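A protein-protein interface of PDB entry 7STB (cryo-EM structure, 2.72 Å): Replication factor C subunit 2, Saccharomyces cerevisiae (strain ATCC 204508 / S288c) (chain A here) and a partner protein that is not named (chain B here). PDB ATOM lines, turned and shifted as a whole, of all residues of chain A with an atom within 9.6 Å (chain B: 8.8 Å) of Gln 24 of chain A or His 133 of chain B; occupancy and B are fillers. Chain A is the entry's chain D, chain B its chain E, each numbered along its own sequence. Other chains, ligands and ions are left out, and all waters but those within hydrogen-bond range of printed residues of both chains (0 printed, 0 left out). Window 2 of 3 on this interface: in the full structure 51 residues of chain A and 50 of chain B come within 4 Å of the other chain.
Of the 21 printed residues of chain B, 7 touch a printed residue of chain A. Along chain B the printed residues that touch a printed residue of chain A span positions 32 to 166. Among the printed residues, 16 pairs touch across the chains.
NE1 of Trp 27 of chain A lies within hydrogen-bond range of OE2 of Glu 208 of chain A (3.2 Å). The side-chain amide oxygen (OE1) of Gln 236 of chain A sits at hydrogen-bond distance from the backbone NH (N) of Trp 27 of chain A. The backbone carbonyl oxygen (O) of Arg 34 of chain B sits at hydrogen-bond distance from the guanidinium group (NH1) of Arg 166 of chain B, 3.2 Å away. The backbone carbonyl oxygen (O) of Leu 36 of chain B lies within hydrogen-bond range of the guanidinium group (NH1) of Arg 166 of chain B. ND1 of His 133 of chain B lies within hydrogen-bond range of O of Gln 121 of chain B, at 2.7 Å. The backbone NH (N) of Arg 166 of chain B lies within hydrogen-bond range of the backbone carbonyl oxygen (O) of Lys 136 of chain B (2.9 Å).
NZ of Lys 163 of chain B lies within hydrogen-bond range of OE1 of Gln 24 of chain A, at 2.8 Å. O of Gln 24 of chain A sits at hydrogen-bond distance from NH2 of Arg 166 of chain B (2.9 Å). The side-chain amide nitrogen of Gln 25 of chain A sits at hydrogen-bond distance from the side-chain hydroxyl of Ser 162 of chain B (3.0 Å). The side-chain amide nitrogen (NE2) of Gln 236 of chain A lies within hydrogen-bond range of the backbone carbonyl oxygen (O) of Asp 35 of chain B, 2.6 Å away. The backbone carbonyl oxygen (O) of Gln 32 of chain B is in hydrogen-bond range of the side-chain amino group (NZ) of Lys 240 of chain A, at 3.4 Å. The side-chain carboxylate (OD1) of Asp 35 of chain B is in salt-bridge range of the side-chain amino group (NZ) of Lys 240 of chain A (2.5 Å). NE2 of Gln 24 of chain A sits close to O of His 133 of chain B (2.4 Å).
Gln 24 of chain A touches just these residues of chain B: Arg 34 (3.8 Å), His 133 (2.4 Å), Lys 163 (2.8 Å) and Arg 166 (2.9 Å). Gln 25 of chain A touches just these residues of chain B: Asp 35 (3.7 Å), Ser 162 (3.0 Å), Lys 163 (2.8 Å) and Arg 166 (3.7 Å). Printed residues of chain B within 4 Å of Trp 27 of chain A: Asp 35. Printed residues of chain B within 4 Å of Lys 240 of chain A: Gln 32 (3.4 Å) and Asp 35 (2.5 Å). Of chain A, only Gln 24 comes within 4 Å of His 133 of chain B. The nearest printed residue of chain A that does not touch Arg 166 of chain B is Pro 26 of chain A (4.1 Å).
Among the printed residues, pairs that only touch across the chains: Ser 21 of chain A with Lys 163 of chain B, Ala 23 of chain A with Arg 34 of chain B, Gln 24 of chain A with Arg 34 of chain B, Gln 25 of chain A with Asp 35 of chain B, Gln 25 of chain A with Lys 163 of chain B, Gln 25 of chain A with Arg 166 of chain B, Pro 26 of chain A with Ser 162 of chain B, Trp 27 of chain A with Asp 35 of chain B and Glu 29 of chain A with Ser 162 of chain B.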
ATOM      1  N   SER A  21     -17.526 -25.544  -2.313  1.00  0.00           N
ATOM      2  CA  SER A  21     -16.131 -25.540  -2.740  1.00  0.00           C
ATOM      3  C   SER A  21     -15.269 -26.398  -1.817  1.00  0.00           C
ATOM      4  O   SER A  21     -14.130 -26.724  -2.146  1.00  0.00           O
ATOM      5  CB  SER A  21     -15.590 -24.110  -2.780  1.00  0.00           C
ATOM      6  OG  SER A  21     -16.265 -23.336  -3.755  1.00  0.00           O
ATOM      7  N   LEU A  22     -15.821 -26.761  -0.656  1.00  0.00           N
ATOM      8  CA  LEU A  22     -15.068 -27.580   0.288  1.00  0.00           C
ATOM      9  C   LEU A  22     -14.730 -28.939  -0.312  1.00  0.00           C
ATOM     10  O   LEU A  22     -13.611 -29.440  -0.139  1.00  0.00           O
ATOM     11  CB  LEU A  22     -15.862 -27.750   1.584  1.00  0.00           C
ATOM     12  CG  LEU A  22     -16.132 -26.470   2.378  1.00  0.00           C
ATOM     13  CD1 LEU A  22     -17.018 -26.765   3.578  1.00  0.00           C
ATOM     14  CD2 LEU A  22     -14.829 -25.819   2.822  1.00  0.00           C
ATOM     15  N   ALA A  23     -15.681 -29.551  -1.016  1.00  0.00           N
ATOM     16  CA  ALA A  23     -15.474 -30.847  -1.652  1.00  0.00           C
ATOM     17  C   ALA A  23     -15.658 -30.791  -3.163  1.00  0.00           C
ATOM     18  O   ALA A  23     -15.765 -31.844  -3.801  1.00  0.00           O
ATOM     19  CB  ALA A  23     -16.423 -31.889  -1.051  1.00  0.00           C
ATOM     20  N   GLN A  24     -15.698 -29.593  -3.753  1.00  0.00           N
ATOM     21  CA  GLN A  24     -15.919 -29.433  -5.185  1.00  0.00           C
ATOM     22  C   GLN A  24     -14.811 -28.627  -5.855  1.00  0.00           C
ATOM     23  O   GLN A  24     -15.022 -28.074  -6.938  1.00  0.00           O
ATOM     24  CB  GLN A  24     -17.275 -28.773  -5.443  1.00  0.00           C
ATOM     25  CG  GLN A  24     -17.994 -29.298  -6.676  1.00  0.00           C
ATOM     26  CD  GLN A  24     -19.276 -28.543  -6.969  1.00  0.00           C
ATOM     27  OE1 GLN A  24     -19.478 -27.429  -6.488  1.00  0.00           O
ATOM     28  NE2 GLN A  24     -20.150 -29.149  -7.765  1.00  0.00           N
ATOM     29  N   GLN A  25     -13.637 -28.545  -5.237  1.00  0.00           N
ATOM     30  CA  GLN A  25     -12.503 -27.831  -5.803  1.00  0.00           C
ATOM     31  C   GLN A  25     -11.242 -28.667  -5.652  1.00  0.00           C
ATOM     32  O   GLN A  25     -11.128 -29.457  -4.707  1.00  0.00           O
ATOM     33  CB  GLN A  25     -12.295 -26.467  -5.126  1.00  0.00           C
ATOM     34  CG  GLN A  25     -13.428 -25.487  -5.357  1.00  0.00           C
ATOM     35  CD  GLN A  25     -13.593 -25.136  -6.821  1.00  0.00           C
ATOM     36  OE1 GLN A  25     -14.563 -25.540  -7.461  1.00  0.00           O
ATOM     37  NE2 GLN A  25     -12.644 -24.381  -7.359  1.00  0.00           N
ATOM     38  N   PRO A  26     -10.278 -28.514  -6.561  1.00  0.00           N
ATOM     39  CA  PRO A  26      -8.993 -29.195  -6.383  1.00  0.00           C
ATOM     40  C   PRO A  26      -8.290 -28.712  -5.124  1.00  0.00           C
ATOM     41  O   PRO A  26      -8.457 -27.570  -4.691  1.00  0.00           O
ATOM     42  CB  PRO A  26      -8.207 -28.820  -7.645  1.00  0.00           C
ATOM     43  CG  PRO A  26      -9.232 -28.393  -8.633  1.00  0.00           C
ATOM     44  CD  PRO A  26     -10.341 -27.786  -7.841  1.00  0.00           C
ATOM     45  N   TRP A  27      -7.494 -29.605  -4.534  1.00  0.00           N
ATOM     46  CA  TRP A  27      -6.829 -29.283  -3.276  1.00  0.00           C
ATOM     47  C   TRP A  27      -5.961 -28.039  -3.410  1.00  0.00           C
ATOM     48  O   TRP A  27      -5.877 -27.228  -2.480  1.00  0.00           O
ATOM     49  CB  TRP A  27      -5.993 -30.473  -2.809  1.00  0.00           C
ATOM     50  CG  TRP A  27      -6.816 -31.621  -2.312  1.00  0.00           C
ATOM     51  CD1 TRP A  27      -8.147 -31.830  -2.529  1.00  0.00           C
ATOM     52  CD2 TRP A  27      -6.363 -32.718  -1.512  1.00  0.00           C
ATOM     53  NE1 TRP A  27      -8.550 -32.990  -1.915  1.00  0.00           N
ATOM     54  CE2 TRP A  27      -7.473 -33.554  -1.284  1.00  0.00           C
ATOM     55  CE3 TRP A  27      -5.126 -33.076  -0.968  1.00  0.00           C
ATOM     56  CZ2 TRP A  27      -7.384 -34.724  -0.535  1.00  0.00           C
ATOM     57  CZ3 TRP A  27      -5.040 -34.238  -0.226  1.00  0.00           C
ATOM     58  CH2 TRP A  27      -6.162 -35.048  -0.016  1.00  0.00           C
ATOM     59  N   GLU A  29      -6.491 -25.451  -5.369  1.00  0.00           N
ATOM     60  CA  GLU A  29      -7.368 -24.288  -5.396  1.00  0.00           C
ATOM     61  C   GLU A  29      -8.103 -24.077  -4.080  1.00  0.00           C
ATOM     62  O   GLU A  29      -8.423 -22.932  -3.741  1.00  0.00           O
ATOM     63  CB  GLU A  29      -8.380 -24.423  -6.536  1.00  0.00           C
ATOM     64  CG  GLU A  29      -9.324 -23.235  -6.686  1.00  0.00           C
ATOM     65  CD  GLU A  29      -8.601 -21.961  -7.081  1.00  0.00           C
ATOM     66  OE1 GLU A  29      -7.520 -22.057  -7.699  1.00  0.00           O
ATOM     67  OE2 GLU A  29      -9.116 -20.865  -6.774  1.00  0.00           O
ATOM     68  N   LYS A  30      -8.383 -25.147  -3.337  1.00  0.00           N
ATOM     69  CA  LYS A  30      -9.098 -25.037  -2.072  1.00  0.00           C
ATOM     70  C   LYS A  30      -8.209 -24.595  -0.918  1.00  0.00           C
ATOM     71  O   LYS A  30      -8.727 -24.076   0.077  1.00  0.00           O
ATOM     72  CB  LYS A  30      -9.751 -26.379  -1.722  1.00  0.00           C
ATOM     73  CG  LYS A  30     -10.675 -26.323  -0.515  1.00  0.00           C
ATOM     74  CD  LYS A  30     -11.261 -27.690  -0.200  1.00  0.00           C
ATOM     75  CE  LYS A  30     -10.330 -28.519   0.667  1.00  0.00           C
ATOM     76  NZ  LYS A  30     -11.048 -29.620   1.365  1.00  0.00           N
ATOM     77  N   GLU A 208      -7.141 -33.093   5.506  1.00  0.00           N
ATOM     78  CA  GLU A 208      -7.748 -34.036   4.575  1.00  0.00           C
ATOM     79  C   GLU A 208      -7.731 -35.471   5.088  1.00  0.00           C
ATOM     80  O   GLU A 208      -8.197 -36.369   4.380  1.00  0.00           O
ATOM     81  CB  GLU A 208      -7.035 -33.970   3.220  1.00  0.00           C
ATOM     82  CG  GLU A 208      -7.262 -32.672   2.469  1.00  0.00           C
ATOM     83  CD  GLU A 208      -8.623 -32.614   1.802  1.00  0.00           C
ATOM     84  OE1 GLU A 208      -9.477 -33.470   2.116  1.00  0.00           O
ATOM     85  OE2 GLU A 208      -8.840 -31.712   0.967  1.00  0.00           O
ATOM     86  N   GLN A 236      -3.068 -35.331  -3.411  1.00  0.00           N
ATOM     87  CA  GLN A 236      -4.474 -35.568  -3.725  1.00  0.00           C
ATOM     88  C   GLN A 236      -4.648 -36.867  -4.500  1.00  0.00           C
ATOM     89  O   GLN A 236      -5.566 -37.650  -4.222  1.00  0.00           O
ATOM     90  CB  GLN A 236      -5.037 -34.391  -4.521  1.00  0.00           C
ATOM     91  CG  GLN A 236      -6.527 -34.488  -4.800  1.00  0.00           C
ATOM     92  CD  GLN A 236      -7.055 -33.288  -5.561  1.00  0.00           C
ATOM     93  OE1 GLN A 236      -6.294 -32.405  -5.954  1.00  0.00           O
ATOM     94  NE2 GLN A 236      -8.365 -33.252  -5.774  1.00  0.00           N
ATOM     95  N   LYS A 240      -6.702 -40.160  -3.281  1.00  0.00           N
ATOM     96  CA  LYS A 240      -7.748 -40.775  -4.092  1.00  0.00           C
ATOM     97  C   LYS A 240      -7.484 -42.263  -4.286  1.00  0.00           C
ATOM     98  O   LYS A 240      -8.400 -43.087  -4.163  1.00  0.00           O
ATOM     99  CB  LYS A 240      -7.842 -40.072  -5.445  1.00  0.00           C
ATOM    100  CG  LYS A 240      -8.545 -38.726  -5.399  1.00  0.00           C
ATOM    101  CD  LYS A 240      -8.707 -38.143  -6.792  1.00  0.00           C
ATOM    102  CE  LYS A 240      -9.645 -36.948  -6.795  1.00  0.00           C
ATOM    103  NZ  LYS A 240     -11.013 -37.302  -6.324  1.00  0.00           N
ATOM    104  N   GLN B  32     -14.707 -40.409  -7.136  1.00  0.00           N
ATOM    105  CA  GLN B  32     -15.266 -39.184  -6.563  1.00  0.00           C
ATOM    106  C   GLN B  32     -15.104 -38.072  -7.592  1.00  0.00           C
ATOM    107  O   GLN B  32     -14.192 -37.241  -7.489  1.00  0.00           O
ATOM    108  CB  GLN B  32     -14.582 -38.824  -5.244  1.00  0.00           C
ATOM    109  CG  GLN B  32     -14.715 -39.888  -4.166  1.00  0.00           C
ATOM    110  CD  GLN B  32     -16.149 -40.090  -3.718  1.00  0.00           C
ATOM    111  OE1 GLN B  32     -16.873 -39.129  -3.461  1.00  0.00           O
ATOM    112  NE2 GLN B  32     -16.568 -41.348  -3.624  1.00  0.00           N
ATOM    113  N   PRO B  33     -15.980 -38.026  -8.606  1.00  0.00           N
ATOM    114  CA  PRO B  33     -15.850 -37.057  -9.703  1.00  0.00           C
ATOM    115  C   PRO B  33     -16.312 -35.646  -9.341  1.00  0.00           C
ATOM    116  O   PRO B  33     -17.161 -35.058 -10.013  1.00  0.00           O
ATOM    117  CB  PRO B  33     -16.724 -37.674 -10.798  1.00  0.00           C
ATOM    118  CG  PRO B  33     -17.785 -38.400 -10.055  1.00  0.00           C
ATOM    119  CD  PRO B  33     -17.152 -38.902  -8.783  1.00  0.00           C
ATOM    120  N   ARG B  34     -15.744 -35.096  -8.268  1.00  0.00           N
ATOM    121  CA  ARG B  34     -16.060 -33.734  -7.853  1.00  0.00           C
ATOM    122  C   ARG B  34     -14.789 -32.909  -7.699  1.00  0.00           C
ATOM    123  O   ARG B  34     -14.775 -31.715  -8.014  1.00  0.00           O
ATOM    124  CB  ARG B  34     -16.850 -33.744  -6.543  1.00  0.00           C
ATOM    125  CG  ARG B  34     -18.276 -34.250  -6.688  1.00  0.00           C
ATOM    126  CD  ARG B  34     -19.045 -34.127  -5.383  1.00  0.00           C
ATOM    127  NE  ARG B  34     -20.394 -34.671  -5.490  1.00  0.00           N
ATOM    128  CZ  ARG B  34     -21.427 -34.022  -6.010  1.00  0.00           C
ATOM    129  NH1 ARG B  34     -21.303 -32.795  -6.491  1.00  0.00           N
ATOM    130  NH2 ARG B  34     -22.615 -34.619  -6.051  1.00  0.00           N
ATOM    131  N   ASP B  35     -13.720 -33.537  -7.220  1.00  0.00           N
ATOM    132  CA  ASP B  35     -12.437 -32.880  -7.007  1.00  0.00           C
ATOM    133  C   ASP B  35     -11.374 -33.457  -7.933  1.00  0.00           C
ATOM    134  O   ASP B  35     -10.218 -33.642  -7.546  1.00  0.00           O
ATOM    135  CB  ASP B  35     -12.001 -33.001  -5.548  1.00  0.00           C
ATOM    136  CG  ASP B  35     -11.947 -34.438  -5.074  1.00  0.00           C
ATOM    137  OD1 ASP B  35     -12.495 -35.317  -5.773  1.00  0.00           O
ATOM    138  OD2 ASP B  35     -11.356 -34.692  -4.003  1.00  0.00           O
ATOM    139  N   LEU B  36     -11.757 -33.751  -9.171  1.00  0.00           N
ATOM    140  CA  LEU B  36     -10.811 -34.277 -10.146  1.00  0.00           C
ATOM    141  C   LEU B  36      -9.939 -33.142 -10.673  1.00  0.00           C
ATOM    142  O   LEU B  36     -10.470 -32.196 -11.264  1.00  0.00           O
ATOM    143  CB  LEU B  36     -11.550 -34.949 -11.296  1.00  0.00           C
ATOM    144  CG  LEU B  36     -10.682 -35.607 -12.370  1.00  0.00           C
ATOM    145  CD1 LEU B  36      -9.858 -36.744 -11.783  1.00  0.00           C
ATOM    146  CD2 LEU B  36     -11.544 -36.108 -13.518  1.00  0.00           C
ATOM    147  N   PHE B  61     -19.839 -38.995 -16.687  1.00  0.00           N
ATOM    148  CA  PHE B  61     -20.999 -38.223 -17.117  1.00  0.00           C
ATOM    149  C   PHE B  61     -22.013 -39.040 -17.910  1.00  0.00           C
ATOM    150  O   PHE B  61     -22.883 -38.456 -18.568  1.00  0.00           O
ATOM    151  CB  PHE B  61     -20.541 -37.021 -17.952  1.00  0.00           C
ATOM    152  CG  PHE B  61     -19.796 -35.970 -17.169  1.00  0.00           C
ATOM    153  CD1 PHE B  61     -19.824 -35.950 -15.784  1.00  0.00           C
ATOM    154  CD2 PHE B  61     -19.056 -35.001 -17.829  1.00  0.00           C
ATOM    155  CE1 PHE B  61     -19.144 -34.983 -15.075  1.00  0.00           C
ATOM    156  CE2 PHE B  61     -18.369 -34.032 -17.120  1.00  0.00           C
ATOM    157  CZ  PHE B  61     -18.412 -34.025 -15.742  1.00  0.00           C
ATOM    158  N   ALA B 117     -15.490 -21.240 -19.951  1.00  0.00           N
ATOM    159  CA  ALA B 117     -15.179 -21.352 -18.530  1.00  0.00           C
ATOM    160  C   ALA B 117     -15.967 -20.338 -17.714  1.00  0.00           C
ATOM    161  O   ALA B 117     -16.436 -20.645 -16.613  1.00  0.00           O
ATOM    162  CB  ALA B 117     -13.678 -21.174 -18.308  1.00  0.00           C
ATOM    163  N   GLN B 118     -16.122 -19.120 -18.238  1.00  0.00           N
ATOM    164  CA  GLN B 118     -16.919 -18.119 -17.539  1.00  0.00           C
ATOM    165  C   GLN B 118     -18.359 -18.588 -17.370  1.00  0.00           C
ATOM    166  O   GLN B 118     -18.963 -18.393 -16.310  1.00  0.00           O
ATOM    167  CB  GLN B 118     -16.870 -16.792 -18.296  1.00  0.00           C
ATOM    168  CG  GLN B 118     -15.515 -16.104 -18.243  1.00  0.00           C
ATOM    169  CD  GLN B 118     -15.322 -15.102 -19.363  1.00  0.00           C
ATOM    170  OE1 GLN B 118     -16.170 -14.968 -20.247  1.00  0.00           O
ATOM    171  NE2 GLN B 118     -14.201 -14.390 -19.334  1.00  0.00           N
ATOM    172  N   MET B 119     -18.923 -19.208 -18.405  1.00  0.00           N
ATOM    173  CA  MET B 119     -20.277 -19.735 -18.309  1.00  0.00           C
ATOM    174  C   MET B 119     -20.341 -20.822 -17.243  1.00  0.00           C
ATOM    175  O   MET B 119     -19.442 -21.661 -17.132  1.00  0.00           O
ATOM    176  CB  MET B 119     -20.721 -20.288 -19.666  1.00  0.00           C
ATOM    177  CG  MET B 119     -22.153 -20.810 -19.707  1.00  0.00           C
ATOM    178  SD  MET B 119     -22.339 -22.489 -19.070  1.00  0.00           S
ATOM    179  CE  MET B 119     -21.579 -23.441 -20.384  1.00  0.00           C
ATOM    180  N   GLU B 120     -21.416 -20.806 -16.460  1.00  0.00           N
ATOM    181  CA  GLU B 120     -21.601 -21.742 -15.359  1.00  0.00           C
ATOM    182  C   GLU B 120     -22.596 -22.821 -15.766  1.00  0.00           C
ATOM    183  O   GLU B 120     -23.680 -22.515 -16.273  1.00  0.00           O
ATOM    184  CB  GLU B 120     -22.095 -21.016 -14.107  1.00  0.00           C
ATOM    185  CG  GLU B 120     -22.167 -21.896 -12.869  1.00  0.00           C
ATOM    186  CD  GLU B 120     -22.411 -21.100 -11.602  1.00  0.00           C
ATOM    187  OE1 GLU B 120     -22.666 -19.882 -11.702  1.00  0.00           O
ATOM    188  OE2 GLU B 120     -22.347 -21.694 -10.504  1.00  0.00           O
ATOM    189  N   GLN B 121     -22.223 -24.077 -15.543  1.00  0.00           N
ATOM    190  CA  GLN B 121     -23.077 -25.205 -15.895  1.00  0.00           C
ATOM    191  C   GLN B 121     -24.098 -25.476 -14.795  1.00  0.00           C
ATOM    192  O   GLN B 121     -23.778 -26.085 -13.774  1.00  0.00           O
ATOM    193  CB  GLN B 121     -22.233 -26.455 -16.150  1.00  0.00           C
ATOM    194  CG  GLN B 121     -22.949 -27.534 -16.946  1.00  0.00           C
ATOM    195  CD  GLN B 121     -22.149 -28.818 -17.039  1.00  0.00           C
ATOM    196  OE1 GLN B 121     -21.189 -29.020 -16.297  1.00  0.00           O
ATOM    197  NE2 GLN B 121     -22.543 -29.695 -17.956  1.00  0.00           N
ATOM    198  N   HIS B 133     -24.682 -28.355  -9.161  1.00  0.00           N
ATOM    199  CA  HIS B 133     -23.744 -27.757 -10.103  1.00  0.00           C
ATOM    200  C   HIS B 133     -22.546 -28.672 -10.333  1.00  0.00           C
ATOM    201  O   HIS B 133     -21.898 -29.113  -9.384  1.00  0.00           O
ATOM    202  CB  HIS B 133     -23.271 -26.393  -9.593  1.00  0.00           C
ATOM    203  CG  HIS B 133     -22.083 -25.854 -10.328  1.00  0.00           C
ATOM    204  ND1 HIS B 133     -22.106 -25.574 -11.678  1.00  0.00           N
ATOM    205  CD2 HIS B 133     -20.837 -25.543  -9.900  1.00  0.00           C
ATOM    206  CE1 HIS B 133     -20.925 -25.114 -12.049  1.00  0.00           C
ATOM    207  NE2 HIS B 133     -20.136 -25.086 -10.989  1.00  0.00           N
ATOM    208  N   ARG B 134     -22.260 -28.952 -11.599  1.00  0.00           N
ATOM    209  CA  ARG B 134     -21.142 -29.793 -12.005  1.00  0.00           C
ATOM    210  C   ARG B 134     -20.229 -29.002 -12.936  1.00  0.00           C
ATOM    211  O   ARG B 134     -20.469 -27.829 -13.231  1.00  0.00           O
ATOM    212  CB  ARG B 134     -21.643 -31.074 -12.680  1.00  0.00           C
ATOM    213  CG  ARG B 134     -22.688 -30.837 -13.758  1.00  0.00           C
ATOM    214  CD  ARG B 134     -23.072 -32.133 -14.452  1.00  0.00           C
ATOM    215  NE  ARG B 134     -23.801 -31.894 -15.692  1.00  0.00           N
ATOM    216  CZ  ARG B 134     -25.094 -31.603 -15.761  1.00  0.00           C
ATOM    217  NH1 ARG B 134     -25.840 -31.501 -14.673  1.00  0.00           N
ATOM    218  NH2 ARG B 134     -25.652 -31.409 -16.953  1.00  0.00           N
ATOM    219  N   TYR B 135     -19.172 -29.660 -13.405  1.00  0.00           N
ATOM    220  CA  TYR B 135     -18.187 -29.044 -14.281  1.00  0.00           C
ATOM    221  C   TYR B 135     -18.200 -29.721 -15.644  1.00  0.00           C
ATOM    222  O   TYR B 135     -18.674 -30.852 -15.791  1.00  0.00           O
ATOM    223  CB  TYR B 135     -16.777 -29.122 -13.678  1.00  0.00           C
ATOM    224  CG  TYR B 135     -16.349 -30.517 -13.279  1.00  0.00           C
ATOM    225  CD1 TYR B 135     -15.965 -31.448 -14.234  1.00  0.00           C
ATOM    226  CD2 TYR B 135     -16.321 -30.898 -11.945  1.00  0.00           C
ATOM    227  CE1 TYR B 135     -15.572 -32.721 -13.873  1.00  0.00           C
ATOM    228  CE2 TYR B 135     -15.929 -32.171 -11.574  1.00  0.00           C
ATOM    229  CZ  TYR B 135     -15.555 -33.076 -12.543  1.00  0.00           C
ATOM    230  OH  TYR B 135     -15.163 -34.344 -12.178  1.00  0.00           O
ATOM    231  N   LYS B 136     -17.675 -29.014 -16.638  1.00  0.00           N
ATOM    232  CA  LYS B 136     -17.511 -29.554 -17.978  1.00  0.00           C
ATOM    233  C   LYS B 136     -16.070 -30.011 -18.178  1.00  0.00           C
ATOM    234  O   LYS B 136     -15.142 -29.501 -17.545  1.00  0.00           O
ATOM    235  CB  LYS B 136     -17.884 -28.509 -19.031  1.00  0.00           C
ATOM    236  CG  LYS B 136     -17.868 -29.026 -20.462  1.00  0.00           C
ATOM    237  CD  LYS B 136     -18.184 -27.923 -21.460  1.00  0.00           C
ATOM    238  CE  LYS B 136     -19.657 -27.550 -21.437  1.00  0.00           C
ATOM    239  NZ  LYS B 136     -19.995 -26.554 -22.491  1.00  0.00           N
ATOM    240  N   TYR B 161     -10.747 -20.606 -13.185  1.00  0.00           N
ATOM    241  CA  TYR B 161     -12.056 -21.184 -13.474  1.00  0.00           C
ATOM    242  C   TYR B 161     -12.071 -22.697 -13.275  1.00  0.00           C
ATOM    243  O   TYR B 161     -12.725 -23.427 -14.021  1.00  0.00           O
ATOM    244  CB  TYR B 161     -12.489 -20.838 -14.895  1.00  0.00           C
ATOM    245  CG  TYR B 161     -12.446 -19.360 -15.207  1.00  0.00           C
ATOM    246  CD1 TYR B 161     -13.398 -18.493 -14.689  1.00  0.00           C
ATOM    247  CD2 TYR B 161     -11.453 -18.831 -16.019  1.00  0.00           C
ATOM    248  CE1 TYR B 161     -13.364 -17.142 -14.973  1.00  0.00           C
ATOM    249  CE2 TYR B 161     -11.409 -17.481 -16.308  1.00  0.00           C
ATOM    250  CZ  TYR B 161     -12.367 -16.641 -15.783  1.00  0.00           C
ATOM    251  OH  TYR B 161     -12.328 -15.296 -16.067  1.00  0.00           O
ATOM    252  N   SER B 162     -11.354 -23.187 -12.263  1.00  0.00           N
ATOM    253  CA  SER B 162     -11.388 -24.614 -11.966  1.00  0.00           C
ATOM    254  C   SER B 162     -12.757 -25.063 -11.474  1.00  0.00           C
ATOM    255  O   SER B 162     -13.078 -26.252 -11.568  1.00  0.00           O
ATOM    256  CB  SER B 162     -10.324 -24.962 -10.924  1.00  0.00           C
ATOM    257  OG  SER B 162     -10.654 -24.422  -9.657  1.00  0.00           O
ATOM    258  N   LYS B 163     -13.569 -24.140 -10.954  1.00  0.00           N
ATOM    259  CA  LYS B 163     -14.911 -24.496 -10.506  1.00  0.00           C
ATOM    260  C   LYS B 163     -15.776 -24.960 -11.671  1.00  0.00           C
ATOM    261  O   LYS B 163     -16.544 -25.921 -11.540  1.00  0.00           O
ATOM    262  CB  LYS B 163     -15.555 -23.298  -9.803  1.00  0.00           C
ATOM    263  CG  LYS B 163     -16.991 -23.513  -9.325  1.00  0.00           C
ATOM    264  CD  LYS B 163     -17.043 -24.258  -8.002  1.00  0.00           C
ATOM    265  CE  LYS B 163     -18.403 -24.117  -7.338  1.00  0.00           C
ATOM    266  NZ  LYS B 163     -18.486 -24.889  -6.067  1.00  0.00           N
ATOM    267  N   ASN B 164     -15.665 -24.293 -12.818  1.00  0.00           N
ATOM    268  CA  ASN B 164     -16.568 -24.538 -13.936  1.00  0.00           C
ATOM    269  C   ASN B 164     -16.089 -25.653 -14.858  1.00  0.00           C
ATOM    270  O   ASN B 164     -16.899 -26.474 -15.300  1.00  0.00           O
ATOM    271  CB  ASN B 164     -16.755 -23.252 -14.745  1.00  0.00           C
ATOM    272  CG  ASN B 164     -17.207 -22.088 -13.889  1.00  0.00           C
ATOM    273  OD1 ASN B 164     -17.923 -22.268 -12.904  1.00  0.00           O
ATOM    274  ND2 ASN B 164     -16.789 -20.883 -14.258  1.00  0.00           N
ATOM    275  N   ILE B 165     -14.796 -25.705 -15.166  1.00  0.00           N
ATOM    276  CA  ILE B 165     -14.268 -26.639 -16.154  1.00  0.00           C
ATOM    277  C   ILE B 165     -13.029 -27.322 -15.602  1.00  0.00           C
ATOM    278  O   ILE B 165     -12.221 -26.704 -14.900  1.00  0.00           O
ATOM    279  CB  ILE B 165     -13.947 -25.932 -17.488  1.00  0.00           C
ATOM    280  CG1 ILE B 165     -15.236 -25.412 -18.126  1.00  0.00           C
ATOM    281  CG2 ILE B 165     -13.212 -26.879 -18.431  1.00  0.00           C
ATOM    282  CD1 ILE B 165     -15.017 -24.581 -19.363  1.00  0.00           C
ATOM    283  N   ARG B 166     -12.884 -28.606 -15.922  1.00  0.00           N
ATOM    284  CA  ARG B 166     -11.678 -29.374 -15.645  1.00  0.00           C
ATOM    285  C   ARG B 166     -11.081 -29.810 -16.974  1.00  0.00           C
ATOM    286  O   ARG B 166     -11.798 -30.307 -17.848  1.00  0.00           O
ATOM    287  CB  ARG B 166     -11.983 -30.585 -14.761  1.00  0.00           C
ATOM    288  CG  ARG B 166     -12.753 -30.257 -13.483  1.00  0.00           C
ATOM    289  CD  ARG B 166     -12.084 -29.165 -12.649  1.00  0.00           C
ATOM    290  NE  ARG B 166     -13.011 -28.555 -11.703  1.00  0.00           N
ATOM    291  CZ  ARG B 166     -13.323 -29.066 -10.520  1.00  0.00           C
ATOM    292  NH1 ARG B 166     -12.803 -30.208 -10.100  1.00  0.00           N
ATOM    293  NH2 ARG B 166     -14.178 -28.414  -9.738  1.00  0.00           N
